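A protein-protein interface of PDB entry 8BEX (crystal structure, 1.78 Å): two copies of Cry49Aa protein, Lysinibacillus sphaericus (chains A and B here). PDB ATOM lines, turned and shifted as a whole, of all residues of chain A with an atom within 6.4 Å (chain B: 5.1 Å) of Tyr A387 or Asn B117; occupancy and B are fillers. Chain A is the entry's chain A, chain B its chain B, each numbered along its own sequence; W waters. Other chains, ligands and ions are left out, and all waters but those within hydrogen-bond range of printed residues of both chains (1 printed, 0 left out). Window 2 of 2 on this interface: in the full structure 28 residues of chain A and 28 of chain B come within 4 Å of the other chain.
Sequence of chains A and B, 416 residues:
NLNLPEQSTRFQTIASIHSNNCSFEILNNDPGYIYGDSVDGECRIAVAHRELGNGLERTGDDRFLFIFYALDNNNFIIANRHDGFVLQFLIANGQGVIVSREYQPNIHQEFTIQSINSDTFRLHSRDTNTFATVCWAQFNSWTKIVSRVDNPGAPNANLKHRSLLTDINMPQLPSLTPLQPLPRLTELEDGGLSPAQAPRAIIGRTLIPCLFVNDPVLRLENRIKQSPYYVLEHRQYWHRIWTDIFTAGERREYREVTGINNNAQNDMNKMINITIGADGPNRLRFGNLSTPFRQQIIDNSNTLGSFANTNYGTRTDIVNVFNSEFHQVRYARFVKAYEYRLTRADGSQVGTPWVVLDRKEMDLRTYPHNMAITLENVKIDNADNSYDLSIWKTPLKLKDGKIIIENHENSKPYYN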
ATOM      1  N   ALA A 278      11.174  31.234   0.038  1.00  0.00           N
ATOM      2  CA  ALA A 278      11.145  31.330  -1.442  1.00  0.00           C
ATOM      3  C   ALA A 278       9.994  32.234  -1.931  1.00  0.00           C
ATOM      4  O   ALA A 278      10.023  32.663  -3.144  1.00  0.00           O
ATOM      5  CB  ALA A 278      11.053  29.944  -2.042  1.00  0.00           C
ATOM      6  N   ASP A 279       9.037  32.565  -1.049  1.00  0.00           N
ATOM      7  CA  ASP A 279       7.833  33.344  -1.435  1.00  0.00           C
ATOM      8  C   ASP A 279       8.161  34.833  -1.515  1.00  0.00           C
ATOM      9  O   ASP A 279       7.338  35.574  -2.081  1.00  0.00           O
ATOM     10  CB  ASP A 279       6.611  33.043  -0.567  1.00  0.00           C
ATOM     11  CG  ASP A 279       6.805  33.072   0.939  1.00  0.00           C
ATOM     12  OD1 ASP A 279       7.991  33.025   1.415  1.00  0.00           O
ATOM     13  OD2 ASP A 279       5.747  33.042   1.638  1.00  0.00           O
ATOM     14  N   GLY A 280       9.337  35.276  -1.073  1.00  0.00           N
ATOM     15  CA  GLY A 280       9.724  36.673  -1.320  1.00  0.00           C
ATOM     16  C   GLY A 280      10.970  37.085  -0.565  1.00  0.00           C
ATOM     17  O   GLY A 280      11.349  36.463   0.449  1.00  0.00           O
ATOM     18  N   PHE A 307       5.330  31.737   4.113  1.00  0.00           N
ATOM     19  CA  PHE A 307       4.414  30.569   4.086  1.00  0.00           C
ATOM     20  C   PHE A 307       5.043  29.379   3.344  1.00  0.00           C
ATOM     21  O   PHE A 307       4.342  28.334   3.197  1.00  0.00           O
ATOM     22  CB  PHE A 307       3.080  30.969   3.445  1.00  0.00           C
ATOM     23  CG  PHE A 307       2.431  32.176   4.080  1.00  0.00           C
ATOM     24  CD1 PHE A 307       2.529  32.404   5.442  1.00  0.00           C
ATOM     25  CD2 PHE A 307       1.703  33.072   3.318  1.00  0.00           C
ATOM     26  CE1 PHE A 307       1.946  33.522   6.026  1.00  0.00           C
ATOM     27  CE2 PHE A 307       1.098  34.178   3.906  1.00  0.00           C
ATOM     28  CZ  PHE A 307       1.225  34.399   5.254  1.00  0.00           C
ATOM     29  N   ALA A 308       6.287  29.528   2.875  1.00  0.00           N
ATOM     30  CA  ALA A 308       6.980  28.531   2.028  1.00  0.00           C
ATOM     31  C   ALA A 308       7.676  27.486   2.913  1.00  0.00           C
ATOM     32  O   ALA A 308       8.119  27.814   4.027  1.00  0.00           O
ATOM     33  CB  ALA A 308       7.943  29.221   1.106  1.00  0.00           C
ATOM     34  N   ASN A 309       7.774  26.265   2.380  1.00  0.00           N
ATOM     35  CA  ASN A 309       8.479  25.101   2.984  1.00  0.00           C
ATOM     36  C   ASN A 309       9.926  25.086   2.460  1.00  0.00           C
ATOM     37  O   ASN A 309      10.694  24.181   2.871  1.00  0.00           O
ATOM     38  CB  ASN A 309       7.745  23.782   2.675  1.00  0.00           C
ATOM     39  CG  ASN A 309       7.248  23.670   1.238  1.00  0.00           C
ATOM     40  OD1 ASN A 309       7.564  24.501   0.368  1.00  0.00           O
ATOM     41  ND2 ASN A 309       6.432  22.662   0.958  1.00  0.00           N
ATOM     42  N   THR A 310      10.291  26.011   1.558  1.00  0.00           N
ATOM     43  CA  THR A 310      11.633  26.023   0.910  1.00  0.00           C
ATOM     44  C   THR A 310      12.245  27.412   1.039  1.00  0.00           C
ATOM     45  O   THR A 310      11.488  28.442   1.093  1.00  0.00           O
ATOM     46  CB  THR A 310      11.596  25.473  -0.527  1.00  0.00           C
ATOM     47  OG1 THR A 310      11.371  26.491  -1.491  1.00  0.00           O
ATOM     48  CG2 THR A 310      10.512  24.444  -0.753  1.00  0.00           C
ATOM     49  N   ASN A 385      15.321  25.813  -7.231  1.00  0.00           N
ATOM     50  CA  ASN A 385      13.983  25.219  -6.967  1.00  0.00           C
ATOM     51  C   ASN A 385      12.981  25.668  -8.042  1.00  0.00           C
ATOM     52  O   ASN A 385      13.327  26.551  -8.918  1.00  0.00           O
ATOM     53  CB  ASN A 385      13.544  25.518  -5.528  1.00  0.00           C
ATOM     54  CG  ASN A 385      13.359  26.994  -5.263  1.00  0.00           C
ATOM     55  OD1 ASN A 385      12.614  27.681  -5.969  1.00  0.00           O
ATOM     56  ND2 ASN A 385      14.058  27.516  -4.262  1.00  0.00           N
ATOM     57  N   SER A 386      11.778  25.102  -7.991  1.00  0.00           N
ATOM     58  CA  SER A 386      10.704  25.368  -8.978  1.00  0.00           C
ATOM     59  C   SER A 386       9.656  26.316  -8.374  1.00  0.00           C
ATOM     60  O   SER A 386       8.571  26.390  -8.940  1.00  0.00           O
ATOM     61  CB  SER A 386      10.095  24.065  -9.483  1.00  0.00           C
ATOM     62  OG  SER A 386       9.539  23.317  -8.406  1.00  0.00           O
ATOM     63  N   TYR A 387       9.969  27.085  -7.326  1.00  0.00           N
ATOM     64  CA  TYR A 387       8.964  27.946  -6.646  1.00  0.00           C
ATOM     65  C   TYR A 387       8.449  29.033  -7.607  1.00  0.00           C
ATOM     66  O   TYR A 387       7.208  29.220  -7.753  1.00  0.00           O
ATOM     67  CB  TYR A 387       9.511  28.570  -5.360  1.00  0.00           C
ATOM     68  CG  TYR A 387       8.407  29.179  -4.534  1.00  0.00           C
ATOM     69  CD1 TYR A 387       7.932  30.462  -4.792  1.00  0.00           C
ATOM     70  CD2 TYR A 387       7.754  28.413  -3.580  1.00  0.00           C
ATOM     71  CE1 TYR A 387       6.867  30.991  -4.073  1.00  0.00           C
ATOM     72  CE2 TYR A 387       6.683  28.923  -2.865  1.00  0.00           C
ATOM     73  CZ  TYR A 387       6.244  30.213  -3.111  1.00  0.00           C
ATOM     74  OH  TYR A 387       5.180  30.686  -2.386  1.00  0.00           O
ATOM     75  N   ASP A 388       9.370  29.717  -8.283  1.00  0.00           N
ATOM     76  CA  ASP A 388       9.066  30.817  -9.226  1.00  0.00           C
ATOM     77  C   ASP A 388       9.770  30.549 -10.549  1.00  0.00           C
ATOM     78  O   ASP A 388      10.992  30.802 -10.627  1.00  0.00           O
ATOM     79  CB  ASP A 388       9.536  32.163  -8.679  1.00  0.00           C
ATOM     80  CG  ASP A 388       9.441  33.289  -9.697  1.00  0.00           C
ATOM     81  OD1 ASP A 388       8.598  33.189 -10.620  1.00  0.00           O
ATOM     82  OD2 ASP A 388      10.205  34.292  -9.541  1.00  0.00           O
ATOM     83  N   LEU A 389       9.035  30.073 -11.551  1.00  0.00           N
ATOM     84  CA  LEU A 389       9.588  29.830 -12.902  1.00  0.00           C
ATOM     85  C   LEU A 389       8.939  30.779 -13.917  1.00  0.00           C
ATOM     86  O   LEU A 389       8.811  30.408 -15.129  1.00  0.00           O
ATOM     87  CB  LEU A 389       9.381  28.355 -13.249  1.00  0.00           C
ATOM     88  CG  LEU A 389      10.168  27.376 -12.376  1.00  0.00           C
ATOM     89  CD1 LEU A 389       9.861  25.950 -12.762  1.00  0.00           C
ATOM     90  CD2 LEU A 389      11.666  27.631 -12.461  1.00  0.00           C
ATOM     91  N   SER B 115       2.579  27.508   1.119  1.00  0.00           N
ATOM     92  CA  SER B 115       2.816  27.828  -0.315  1.00  0.00           C
ATOM     93  C   SER B 115       3.738  26.776  -0.923  1.00  0.00           C
ATOM     94  O   SER B 115       4.887  26.646  -0.431  1.00  0.00           O
ATOM     95  CB  SER B 115       3.396  29.182  -0.527  1.00  0.00           C
ATOM     96  OG  SER B 115       2.526  30.158  -0.015  1.00  0.00           O
ATOM     97  N   ILE B 116       3.257  26.101  -1.976  1.00  0.00           N
ATOM     98  CA  ILE B 116       4.020  25.105  -2.781  1.00  0.00           C
ATOM     99  C   ILE B 116       4.828  25.863  -3.830  1.00  0.00           C
ATOM    100  O   ILE B 116       5.957  25.428  -4.138  1.00  0.00           O
ATOM    101  CB  ILE B 116       3.051  24.094  -3.438  1.00  0.00           C
ATOM    102  CG1 ILE B 116       2.112  23.452  -2.411  1.00  0.00           C
ATOM    103  CG2 ILE B 116       3.807  23.049  -4.234  1.00  0.00           C
ATOM    104  CD1 ILE B 116       2.850  22.695  -1.315  1.00  0.00           C
ATOM    105  N   ASN B 117       4.216  26.896  -4.417  1.00  0.00           N
ATOM    106  CA  ASN B 117       4.826  27.777  -5.444  1.00  0.00           C
ATOM    107  C   ASN B 117       3.996  29.063  -5.495  1.00  0.00           C
ATOM    108  O   ASN B 117       3.126  29.239  -4.621  1.00  0.00           O
ATOM    109  CB  ASN B 117       5.002  27.063  -6.792  1.00  0.00           C
ATOM    110  CG  ASN B 117       3.734  26.461  -7.368  1.00  0.00           C
ATOM    111  OD1 ASN B 117       3.780  25.349  -7.889  1.00  0.00           O
ATOM    112  ND2 ASN B 117       2.623  27.174  -7.307  1.00  0.00           N
ATOM    113  N   SER B 118       4.276  29.952  -6.447  1.00  0.00           N
ATOM    114  CA  SER B 118       3.819  31.370  -6.448  1.00  0.00           C
ATOM    115  C   SER B 118       2.294  31.485  -6.328  1.00  0.00           C
ATOM    116  O   SER B 118       1.829  32.366  -5.569  1.00  0.00           O
ATOM    117  CB  SER B 118       4.307  32.082  -7.672  1.00  0.00           C
ATOM    118  OG  SER B 118       5.707  31.895  -7.838  1.00  0.00           O
ATOM    119  N   ASP B 119       1.531  30.627  -7.021  1.00  0.00           N
ATOM    120  CA  ASP B 119       0.049  30.755  -7.174  1.00  0.00           C
ATOM    121  C   ASP B 119      -0.693  29.539  -6.568  1.00  0.00           C
ATOM    122  O   ASP B 119      -1.943  29.483  -6.707  1.00  0.00           O
ATOM    123  CB  ASP B 119      -0.294  30.934  -8.662  1.00  0.00           C
ATOM    124  CG  ASP B 119       0.348  29.853  -9.517  1.00  0.00           C
ATOM    125  OD1 ASP B 119       0.252  28.682  -9.103  1.00  0.00           O
ATOM    126  OD2 ASP B 119       0.979  30.179 -10.565  1.00  0.00           O
ATOM    127  N   THR B 120       0.019  28.606  -5.922  1.00  0.00           N
ATOM    128  CA  THR B 120      -0.534  27.348  -5.357  1.00  0.00           C
ATOM    129  C   THR B 120      -0.204  27.248  -3.873  1.00  0.00           C
ATOM    130  O   THR B 120       0.993  27.471  -3.487  1.00  0.00           O
ATOM    131  CB  THR B 120       0.026  26.100  -6.049  1.00  0.00           C
ATOM    132  OG1 THR B 120      -0.082  26.329  -7.447  1.00  0.00           O
ATOM    133  CG2 THR B 120      -0.718  24.840  -5.683  1.00  0.00           C
HETATM  134  O   HOH W   1       3.402  32.856   0.279  1.00  0.00           O
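The backbone NH of Phe A307 sits at hydrogen-bond distance from the side-chain carboxylate of Asp A279, 2.8 Å away.
N of Tyr A387 lies within hydrogen-bond range of OD1 of Asn A385.
The side-chain amide nitrogen (ND2) of Asn B117 lies within hydrogen-bond range of the side-chain hydroxyl (OG1) of Thr B120, at 2.8 Å.
The side-chain amide nitrogen of Asn B117 is in hydrogen-bond range of the side-chain carboxylate of Asp B119, 3.3 Å away.
Water W1 lies within hydrogen-bond range of OD2 of Asp A279 (2.7 Å) and OG of Ser B115 (2.9 Å).
O of Tyr A387 is in hydrogen-bond range of OG of Ser B118, at 3.1 Å.
O of Asn B117 sits at hydrogen-bond distance from OH of Tyr A387, 3.4 Å away.
O of Phe A307 is in hydrogen-bond range of N of Ser B115, 2.8 Å away.
Of the 12 printed residues of chain A, 5 touch a printed residue of chain B.
Along chain A the printed residues that touch a printed residue of chain B span positions 307 to 388.
Among the printed residues, 8 pairs touch across the chains.
Among the printed residues, no Asp or Glu carboxylate lies within 4 Å of a Lys or Arg side-chain nitrogen of the other chain.
Among the printed residues, pairs that only touch across the chains: Ala A308 with Ser B115, Asn A309 with Ser B115, Tyr A387 with Ser B115, Tyr A387 with Ile B116 and Asp A388 with Ser B118.
No position is printed for both chains.
Of the 8 pairs that touch across the chains among the printed residues, none has its exchanged pair printed and touching as well.
Of chain B, only Ser B115, Ile B116, Asn B117 and Ser B118 come within 4 Å of Tyr A387.
Asn B117 touches one residue of chain A.
Of the printed residues of chain B, Phe A307 touches Ser B115 (2.8 Å).
Printed residues of chain B within 4 Å of Asp A388: Ser B118 (3.8 Å).
Of the printed residues of chain B, Asn A309 touches Ser B115.
Of the printed residues of chain A, Ser B118 touches Tyr A387 (3.1 Å) and Asp A388 (3.8 Å).
Gly A280 touches none of the printed residues of chain B.
The nearest printed residue of chain B that does not touch Tyr A387 is Thr B120 (5.4 Å).
The nearest residue of chain A that does not touch Asn B117 is Ser A386 (4.2 Å).
The nearest printed residue of chain A that does not touch Ser B115 is Asp A279 (4.6 Å).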
